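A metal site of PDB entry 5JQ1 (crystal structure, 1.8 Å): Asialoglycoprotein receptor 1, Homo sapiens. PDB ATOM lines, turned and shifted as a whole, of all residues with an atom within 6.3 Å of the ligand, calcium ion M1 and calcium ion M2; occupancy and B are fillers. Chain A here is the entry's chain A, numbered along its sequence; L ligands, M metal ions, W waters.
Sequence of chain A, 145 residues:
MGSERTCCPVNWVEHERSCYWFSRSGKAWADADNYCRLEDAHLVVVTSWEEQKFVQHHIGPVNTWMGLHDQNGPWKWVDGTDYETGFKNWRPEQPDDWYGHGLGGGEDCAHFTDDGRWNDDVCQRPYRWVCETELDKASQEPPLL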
ATOM      1  N   ASN A  63      25.388 -31.621 -13.783  1.00  0.00           N
ATOM      2  CA  ASN A  63      25.987 -30.276 -13.604  1.00  0.00           C
ATOM      3  C   ASN A  63      27.293 -30.238 -14.339  1.00  0.00           C
ATOM      4  O   ASN A  63      28.122 -31.125 -14.140  1.00  0.00           O
ATOM      5  CB  ASN A  63      26.175 -29.914 -12.138  1.00  0.00           C
ATOM      6  CG  ASN A  63      24.885 -29.758 -11.373  1.00  0.00           C
ATOM      7  OD1 ASN A  63      24.748 -30.173 -10.221  1.00  0.00           O
ATOM      8  ND2 ASN A  63      23.961 -29.065 -11.948  1.00  0.00           N
ATOM      9  N   ASP A  70      31.593 -14.379 -13.791  1.00  0.00           N
ATOM     10  CA  ASP A  70      31.613 -12.957 -13.433  1.00  0.00           C
ATOM     11  C   ASP A  70      32.681 -12.716 -12.361  1.00  0.00           C
ATOM     12  O   ASP A  70      32.539 -11.829 -11.513  1.00  0.00           O
ATOM     13  CB  ASP A  70      30.205 -12.467 -12.963  1.00  0.00           C
ATOM     14  CG  ASP A  70      29.770 -12.921 -11.586  1.00  0.00           C
ATOM     15  OD1 ASP A  70      30.277 -13.960 -11.109  1.00  0.00           O
ATOM     16  OD2 ASP A  70      28.901 -12.254 -10.985  1.00  0.00           O
ATOM     17  N   GLN A  71      33.786 -13.478 -12.450  1.00  0.00           N
ATOM     18  CA  GLN A  71      34.904 -13.349 -11.509  1.00  0.00           C
ATOM     19  C   GLN A  71      35.557 -11.963 -11.502  1.00  0.00           C
ATOM     20  O   GLN A  71      36.086 -11.577 -10.469  1.00  0.00           O
ATOM     21  CB  GLN A  71      35.979 -14.430 -11.728  1.00  0.00           C
ATOM     22  CG  GLN A  71      35.449 -15.842 -11.604  1.00  0.00           C
ATOM     23  CD  GLN A  71      36.546 -16.835 -11.797  1.00  0.00           C
ATOM     24  OE1 GLN A  71      36.802 -17.297 -12.904  1.00  0.00           O
ATOM     25  NE2 GLN A  71      37.187 -17.216 -10.707  1.00  0.00           N
ATOM     26  N   GLY A  73      33.917  -9.062 -12.471  1.00  0.00           N
ATOM     27  CA  GLY A  73      32.868  -8.052 -12.402  1.00  0.00           C
ATOM     28  C   GLY A  73      31.651  -8.480 -13.160  1.00  0.00           C
ATOM     29  O   GLY A  73      30.800  -9.184 -12.613  1.00  0.00           O
ATOM     30  N   TRP A  75      29.294 -10.384 -16.121  1.00  0.00           N
ATOM     31  CA  TRP A  75      29.269 -11.682 -16.813  1.00  0.00           C
ATOM     32  C   TRP A  75      30.098 -11.594 -18.120  1.00  0.00           C
ATOM     33  O   TRP A  75      29.954 -10.637 -18.880  1.00  0.00           O
ATOM     34  CB  TRP A  75      27.821 -12.111 -17.135  1.00  0.00           C
ATOM     35  CG  TRP A  75      27.121 -12.605 -15.899  1.00  0.00           C
ATOM     36  CD1 TRP A  75      26.202 -11.930 -15.150  1.00  0.00           C
ATOM     37  CD2 TRP A  75      27.439 -13.793 -15.166  1.00  0.00           C
ATOM     38  NE1 TRP A  75      25.854 -12.678 -14.046  1.00  0.00           N
ATOM     39  CE2 TRP A  75      26.627 -13.803 -14.007  1.00  0.00           C
ATOM     40  CE3 TRP A  75      28.303 -14.878 -15.396  1.00  0.00           C
ATOM     41  CZ2 TRP A  75      26.690 -14.848 -13.060  1.00  0.00           C
ATOM     42  CZ3 TRP A  75      28.370 -15.901 -14.455  1.00  0.00           C
ATOM     43  CH2 TRP A  75      27.577 -15.861 -13.290  1.00  0.00           C
ATOM     44  N   ARG A  91      18.335 -20.724 -15.275  1.00  0.00           N
ATOM     45  CA  ARG A  91      17.248 -21.386 -14.561  1.00  0.00           C
ATOM     46  C   ARG A  91      16.420 -20.264 -13.857  1.00  0.00           C
ATOM     47  O   ARG A  91      16.974 -19.185 -13.561  1.00  0.00           O
ATOM     48  CB  ARG A  91      17.836 -22.373 -13.513  1.00  0.00           C
ATOM     49  CG  ARG A  91      17.234 -23.764 -13.658  1.00  0.00           C
ATOM     50  CD  ARG A  91      17.675 -24.678 -12.563  1.00  0.00           C
ATOM     51  NE  ARG A  91      16.589 -25.538 -12.098  1.00  0.00           N
ATOM     52  CZ  ARG A  91      16.586 -26.861 -12.193  1.00  0.00           C
ATOM     53  NH1 ARG A  91      17.617 -27.492 -12.767  1.00  0.00           N
ATOM     54  NH2 ARG A  91      15.576 -27.568 -11.723  1.00  0.00           N
ATOM     55  N   GLU A  93      15.080 -17.773 -11.098  1.00  0.00           N
ATOM     56  CA  GLU A  93      15.698 -17.249  -9.872  1.00  0.00           C
ATOM     57  C   GLU A  93      17.237 -17.282  -9.946  1.00  0.00           C
ATOM     58  O   GLU A  93      17.893 -17.035  -8.941  1.00  0.00           O
ATOM     59  CB  GLU A  93      15.202 -17.956  -8.578  1.00  0.00           C
ATOM     60  CG  GLU A  93      13.698 -17.871  -8.335  1.00  0.00           C
ATOM     61  CD  GLU A  93      13.290 -18.393  -6.963  1.00  0.00           C
ATOM     62  OE1 GLU A  93      12.924 -17.564  -6.110  1.00  0.00           O
ATOM     63  OE2 GLU A  93      13.410 -19.621  -6.731  1.00  0.00           O
ATOM     64  N   GLN A  94      17.803 -17.579 -11.126  1.00  0.00           N
ATOM     65  CA  GLN A  94      19.257 -17.512 -11.301  1.00  0.00           C
ATOM     66  C   GLN A  94      19.595 -16.404 -12.323  1.00  0.00           C
ATOM     67  O   GLN A  94      18.762 -16.104 -13.186  1.00  0.00           O
ATOM     68  CB  GLN A  94      19.855 -18.872 -11.754  1.00  0.00           C
ATOM     69  CG  GLN A  94      19.563 -20.052 -10.821  1.00  0.00           C
ATOM     70  CD  GLN A  94      20.022 -19.860  -9.388  1.00  0.00           C
ATOM     71  OE1 GLN A  94      20.989 -19.103  -9.088  1.00  0.00           O
ATOM     72  NE2 GLN A  94      19.408 -20.661  -8.515  1.00  0.00           N
ATOM     73  N   PRO A  95      20.823 -15.859 -12.313  1.00  0.00           N
ATOM     74  CA  PRO A  95      21.899 -16.086 -11.325  1.00  0.00           C
ATOM     75  C   PRO A  95      21.558 -15.348 -10.024  1.00  0.00           C
ATOM     76  O   PRO A  95      20.837 -14.332 -10.050  1.00  0.00           O
ATOM     77  CB  PRO A  95      23.142 -15.535 -12.035  1.00  0.00           C
ATOM     78  CG  PRO A  95      22.619 -14.448 -12.971  1.00  0.00           C
ATOM     79  CD  PRO A  95      21.181 -14.799 -13.293  1.00  0.00           C
ATOM     80  N   ASP A  96      22.042 -15.822  -8.895  1.00  0.00           N
ATOM     81  CA  ASP A  96      21.693 -15.160  -7.635  1.00  0.00           C
ATOM     82  C   ASP A  96      22.895 -14.821  -6.737  1.00  0.00           C
ATOM     83  O   ASP A  96      22.690 -14.281  -5.635  1.00  0.00           O
ATOM     84  CB  ASP A  96      20.651 -16.004  -6.887  1.00  0.00           C
ATOM     85  CG  ASP A  96      21.210 -17.368  -6.442  1.00  0.00           C
ATOM     86  OD1 ASP A  96      22.356 -17.696  -6.837  1.00  0.00           O
ATOM     87  OD2 ASP A  96      20.503 -18.089  -5.748  1.00  0.00           O
ATOM     88  N   ASP A  97      24.123 -15.164  -7.166  1.00  0.00           N
ATOM     89  CA  ASP A  97      25.369 -14.919  -6.403  1.00  0.00           C
ATOM     90  C   ASP A  97      25.235 -15.342  -4.928  1.00  0.00           C
ATOM     91  O   ASP A  97      25.510 -14.559  -4.019  1.00  0.00           O
ATOM     92  CB  ASP A  97      25.725 -13.423  -6.491  1.00  0.00           C
ATOM     93  CG  ASP A  97      27.168 -13.076  -6.147  1.00  0.00           C
ATOM     94  OD1 ASP A  97      28.091 -13.805  -6.581  1.00  0.00           O
ATOM     95  OD2 ASP A  97      27.374 -12.079  -5.424  1.00  0.00           O
ATOM     96  N   TRP A  98      24.681 -16.522  -4.697  1.00  0.00           N
ATOM     97  CA  TRP A  98      24.391 -17.022  -3.342  1.00  0.00           C
ATOM     98  C   TRP A  98      25.663 -17.118  -2.470  1.00  0.00           C
ATOM     99  O   TRP A  98      26.664 -17.675  -2.915  1.00  0.00           O
ATOM    100  CB  TRP A  98      23.685 -18.394  -3.452  1.00  0.00           C
ATOM    101  CG  TRP A  98      23.148 -18.953  -2.162  1.00  0.00           C
ATOM    102  CD1 TRP A  98      22.290 -18.347  -1.287  1.00  0.00           C
ATOM    103  CD2 TRP A  98      23.331 -20.310  -1.694  1.00  0.00           C
ATOM    104  NE1 TRP A  98      21.962 -19.229  -0.274  1.00  0.00           N
ATOM    105  CE2 TRP A  98      22.587 -20.429  -0.492  1.00  0.00           C
ATOM    106  CE3 TRP A  98      24.079 -21.409  -2.148  1.00  0.00           C
ATOM    107  CZ2 TRP A  98      22.541 -21.636   0.228  1.00  0.00           C
ATOM    108  CZ3 TRP A  98      24.047 -22.590  -1.426  1.00  0.00           C
ATOM    109  CH2 TRP A  98      23.317 -22.682  -0.222  1.00  0.00           C
ATOM    110  N   GLY A 106      30.510 -15.221  -3.170  1.00  0.00           N
ATOM    111  CA  GLY A 106      29.192 -15.507  -3.739  1.00  0.00           C
ATOM    112  C   GLY A 106      29.279 -16.710  -4.674  1.00  0.00           C
ATOM    113  O   GLY A 106      29.726 -17.794  -4.262  1.00  0.00           O
ATOM    114  N   GLU A 107      28.831 -16.551  -5.911  1.00  0.00           N
ATOM    115  CA  GLU A 107      28.864 -17.639  -6.924  1.00  0.00           C
ATOM    116  C   GLU A 107      29.214 -16.979  -8.223  1.00  0.00           C
ATOM    117  O   GLU A 107      28.491 -16.079  -8.643  1.00  0.00           O
ATOM    118  CB  GLU A 107      27.494 -18.305  -7.034  1.00  0.00           C
ATOM    119  CG  GLU A 107      27.243 -19.289  -5.918  1.00  0.00           C
ATOM    120  CD  GLU A 107      25.853 -19.850  -5.919  1.00  0.00           C
ATOM    121  OE1 GLU A 107      25.680 -20.965  -5.367  1.00  0.00           O
ATOM    122  OE2 GLU A 107      24.933 -19.191  -6.464  1.00  0.00           O
ATOM    123  N   ASP A 108      30.359 -17.358  -8.832  1.00  0.00           N
ATOM    124  CA  ASP A 108      30.849 -16.620  -9.989  1.00  0.00           C
ATOM    125  C   ASP A 108      30.997 -17.390 -11.304  1.00  0.00           C
ATOM    126  O   ASP A 108      31.460 -16.786 -12.267  1.00  0.00           O
ATOM    127  CB  ASP A 108      32.217 -15.978  -9.612  1.00  0.00           C
ATOM    128  CG  ASP A 108      32.166 -14.998  -8.444  1.00  0.00           C
ATOM    129  OD1 ASP A 108      31.049 -14.615  -8.036  1.00  0.00           O
ATOM    130  OD2 ASP A 108      33.224 -14.510  -8.040  1.00  0.00           O
ATOM    131  N   CYS A 109      30.691 -18.714 -11.329  1.00  0.00           N
ATOM    132  CA  CYS A 109      30.907 -19.567 -12.495  1.00  0.00           C
ATOM    133  C   CYS A 109      29.607 -20.211 -12.970  1.00  0.00           C
ATOM    134  O   CYS A 109      28.855 -20.738 -12.167  1.00  0.00           O
ATOM    135  CB  CYS A 109      31.994 -20.608 -12.196  1.00  0.00           C
ATOM    136  SG  CYS A 109      33.667 -19.914 -12.049  1.00  0.00           S
ATOM    137  N   HIS A 111      27.198 -22.992 -14.893  1.00  0.00           N
ATOM    138  CA  HIS A 111      27.132 -24.382 -15.287  1.00  0.00           C
ATOM    139  C   HIS A 111      25.724 -24.724 -15.791  1.00  0.00           C
ATOM    140  O   HIS A 111      24.752 -24.104 -15.386  1.00  0.00           O
ATOM    141  CB  HIS A 111      27.554 -25.338 -14.117  1.00  0.00           C
ATOM    142  CG  HIS A 111      26.597 -25.392 -12.953  1.00  0.00           C
ATOM    143  ND1 HIS A 111      25.625 -26.391 -12.856  1.00  0.00           N
ATOM    144  CD2 HIS A 111      26.503 -24.576 -11.872  1.00  0.00           C
ATOM    145  CE1 HIS A 111      24.992 -26.146 -11.719  1.00  0.00           C
ATOM    146  NE2 HIS A 111      25.447 -25.057 -11.116  1.00  0.00           N
ATOM    147  N   THR A 113      22.573 -26.977 -15.509  1.00  0.00           N
ATOM    148  CA  THR A 113      21.996 -27.794 -14.438  1.00  0.00           C
ATOM    149  C   THR A 113      21.428 -29.091 -15.048  1.00  0.00           C
ATOM    150  O   THR A 113      21.526 -29.306 -16.268  1.00  0.00           O
ATOM    151  CB  THR A 113      20.895 -27.053 -13.669  1.00  0.00           C
ATOM    152  OG1 THR A 113      19.831 -26.781 -14.576  1.00  0.00           O
ATOM    153  CG2 THR A 113      21.397 -25.782 -12.994  1.00  0.00           C
ATOM    154  N   ASN A 119      22.931 -22.106 -13.990  1.00  0.00           N
ATOM    155  CA  ASN A 119      23.067 -21.684 -12.608  1.00  0.00           C
ATOM    156  C   ASN A 119      24.456 -21.108 -12.404  1.00  0.00           C
ATOM    157  O   ASN A 119      25.389 -21.568 -13.034  1.00  0.00           O
ATOM    158  CB  ASN A 119      22.854 -22.865 -11.651  1.00  0.00           C
ATOM    159  CG  ASN A 119      23.029 -22.469 -10.204  1.00  0.00           C
ATOM    160  OD1 ASN A 119      22.537 -21.434  -9.768  1.00  0.00           O
ATOM    161  ND2 ASN A 119      23.924 -23.145  -9.517  1.00  0.00           N
ATOM    162  N   ASP A 120      24.600 -20.121 -11.505  1.00  0.00           N
ATOM    163  CA  ASP A 120      25.921 -19.609 -11.121  1.00  0.00           C
ATOM    164  C   ASP A 120      26.270 -20.376  -9.828  1.00  0.00           C
ATOM    165  O   ASP A 120      25.415 -20.567  -8.970  1.00  0.00           O
ATOM    166  CB  ASP A 120      25.918 -18.091 -10.869  1.00  0.00           C
ATOM    167  CG  ASP A 120      24.941 -17.570  -9.835  1.00  0.00           C
ATOM    168  OD1 ASP A 120      23.827 -18.170  -9.686  1.00  0.00           O
ATOM    169  OD2 ASP A 120      25.188 -16.457  -9.313  1.00  0.00           O
ATOM    170  N   ASP A 121      27.495 -20.884  -9.725  1.00  0.00           N
ATOM    171  CA  ASP A 121      27.920 -21.655  -8.553  1.00  0.00           C
ATOM    172  C   ASP A 121      29.338 -21.276  -8.174  1.00  0.00           C
ATOM    173  O   ASP A 121      30.014 -20.508  -8.857  1.00  0.00           O
ATOM    174  CB  ASP A 121      27.807 -23.196  -8.839  1.00  0.00           C
ATOM    175  CG  ASP A 121      27.460 -24.038  -7.628  1.00  0.00           C
ATOM    176  OD1 ASP A 121      27.764 -23.611  -6.492  1.00  0.00           O
ATOM    177  OD2 ASP A 121      26.771 -25.087  -7.804  1.00  0.00           O
ATOM    178  N   VAL A 122      29.793 -21.850  -7.067  1.00  0.00           N
ATOM    179  CA  VAL A 122      31.112 -21.651  -6.506  1.00  0.00           C
ATOM    180  C   VAL A 122      32.106 -22.241  -7.492  1.00  0.00           C
ATOM    181  O   VAL A 122      32.043 -23.440  -7.802  1.00  0.00           O
ATOM    182  CB  VAL A 122      31.130 -22.338  -5.120  1.00  0.00           C
ATOM    183  CG1 VAL A 122      32.509 -22.276  -4.487  1.00  0.00           C
ATOM    184  CG2 VAL A 122      30.093 -21.700  -4.195  1.00  0.00           C
ATOM    185  N   TYR A 127      32.960 -30.115 -11.227  1.00  0.00           N
ATOM    186  CA  TYR A 127      31.890 -30.537 -12.105  1.00  0.00           C
ATOM    187  C   TYR A 127      32.530 -30.975 -13.389  1.00  0.00           C
ATOM    188  O   TYR A 127      33.670 -30.577 -13.706  1.00  0.00           O
ATOM    189  CB  TYR A 127      30.932 -29.350 -12.455  1.00  0.00           C
ATOM    190  CG  TYR A 127      29.954 -28.890 -11.405  1.00  0.00           C
ATOM    191  CD1 TYR A 127      29.360 -29.800 -10.525  1.00  0.00           C
ATOM    192  CD2 TYR A 127      29.506 -27.574 -11.380  1.00  0.00           C
ATOM    193  CE1 TYR A 127      28.422 -29.393  -9.569  1.00  0.00           C
ATOM    194  CE2 TYR A 127      28.592 -27.138 -10.422  1.00  0.00           C
ATOM    195  CZ  TYR A 127      28.034 -28.056  -9.534  1.00  0.00           C
ATOM    196  OH  TYR A 127      27.062 -27.616  -8.666  1.00  0.00           O
HETATM  197  C1  LIG L   1      22.729 -22.483  -5.965  1.00  0.00           C
HETATM  198  C2  LIG L   1      21.017 -23.278  -3.671  1.00  0.00           C
HETATM  199  C3  LIG L   1      20.624 -22.036  -4.576  1.00  0.00           C
HETATM  200  C4  LIG L   1      19.769 -20.935  -3.884  1.00  0.00           C
HETATM  201  C5  LIG L   1      20.551 -23.879  -5.877  1.00  0.00           C
HETATM  202  O1  LIG L   1      21.555 -25.285  -8.829  1.00  0.00           O
HETATM  203  C6  LIG L   1      22.434 -25.538  -8.055  1.00  0.00           C
HETATM  204  C7  LIG L   1      23.342 -26.754  -8.171  1.00  0.00           C
HETATM  205  N1  LIG L   1      22.640 -24.702  -6.967  1.00  0.00           N
HETATM  206  C8  LIG L   1      21.843 -23.504  -6.712  1.00  0.00           C
HETATM  207  O2  LIG L   1      23.700 -21.989  -6.831  1.00  0.00           O
HETATM  208  C9  LIG L   1      21.870 -21.376  -5.284  1.00  0.00           C
HETATM  209  O3  LIG L   1      21.490 -20.512  -6.351  1.00  0.00           O
HETATM  210  O4  LIG L   1      18.541 -21.428  -3.493  1.00  0.00           O
HETATM  211  O5  LIG L   1      19.859 -22.664  -5.595  1.00  0.00           O
HETATM  212  O6  LIG L   1      20.903 -24.389  -4.591  1.00  0.00           O
HETATM  213 CA    CA M   1      23.164 -19.775  -8.023  1.00  0.00          CA
HETATM  214 CA    CA M   2      28.846 -13.635  -8.899  1.00  0.00          CA
HETATM  215  O   HOH W   1      27.445 -11.392  -8.740  1.00  0.00           O
HETATM  216  O   HOH W   2      25.286 -25.318  -5.556  1.00  0.00           O
HETATM  217  O   HOH W   3      26.632 -14.171  -9.712  1.00  0.00           O
HETATM  218  O   HOH W   4      20.117 -27.523  -9.960  1.00  0.00           O
HETATM  219  O   HOH W   5      19.580 -23.869 -10.007  1.00  0.00           O
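OD2 of Asp 120 sits at hydrogen-bond distance from N of Asp 97 (2.7 Å).
The side-chain carboxylate (OE2) of Glu 107 lies close to the backbone NH (N) of Trp 98 (3.2 Å).
A ring nitrogen (NE2) of His 111 is in hydrogen-bond range of the side-chain amide nitrogen (ND2) of Asn 119, at 2.9 Å.
The side-chain carboxylate (OD1) of Asp 96 sits close to the backbone NH (N) of Trp 98.
O of Asp 121 is in hydrogen-bond range of N of Asp 108 (3.2 Å).
The side-chain carboxylate (OD2) of Asp 121 sits at hydrogen-bond distance from the side-chain hydroxyl (OH) of Tyr 127 (2.7 Å).
The backbone carbonyl oxygen of Cys 109 sits at hydrogen-bond distance from the backbone NH of Asp 121, at 2.8 Å.
The side-chain amide nitrogen (ND2) of Asn 63 lies close to a ring nitrogen (ND1) of His 111, at 3.3 Å.
Trp 98 touches the ligand (CZ3 to C2, 3.8 Å).
CE1 of His 111 touches C7 of the ligand (3.96 Å).
Asp 121 touches the ligand (OD2 to C7, 3.8 Å).
Tyr 127 touches the ligand (OH to C7, 3.9 Å).
Hydrophobic or aromatic side chains within 4 Å of the ligand: Trp 98 and His 111.
Within 4 Å of the ligand: Gln 94, Asp 96, Trp 98, Glu 107, His 111, Asn 119, Asp 120, Asp 121 and Tyr 127.
Of the 23 residues printed, 5 come within 4 Å of calcium ion M1.
The nearest printed residue that does not touch calcium ion M1 is Asp 121 (4.8 Å).
Along chain A the residues within 4 Å of calcium ion M2 span positions 70 to 108.
Calcium ion M1 is bound by the side-chain carboxylate (OD1) of Asp 120 (2.4 Å), the side-chain carboxylate (OE2) of Glu 107 (2.4 Å), an oxygen (O3) of the ligand (2.5 Å), the side-chain amide oxygen (OD1) of Asn 119 (2.5 Å), the side-chain amide oxygen (OE1) of Gln 94 (2.5 Å), the side-chain carboxylate (OD1) of Asp 96 (2.5 Å), the backbone carbonyl oxygen (O) of Asp 120 (2.6 Å) and an oxygen (O2) of the ligand (2.6 Å).
Calcium ion M1 has eight donor atoms within binding distance.
Calcium ion M2 is bound by water W3 (2.4 Å).
Calcium ion M2 is bound by OD1 of Asp 97, 2.4 Å away.
Calcium ion M2 is bound by O of Glu 107, at 2.5 Å.
Calcium ion M2 is bound by the side-chain carboxylate (OD2) of Asp 70 (2.5 Å).
OD1 of Asp 108 is bound to calcium ion M2.
Water W1 binds calcium ion M2.
OD1 of Asp 70 binds calcium ion M2, 2.7 Å away.
Water W2 bridges the side-chain carboxylate (OD2) of Asp 121 and a nitrogen (N1) of the ligand.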
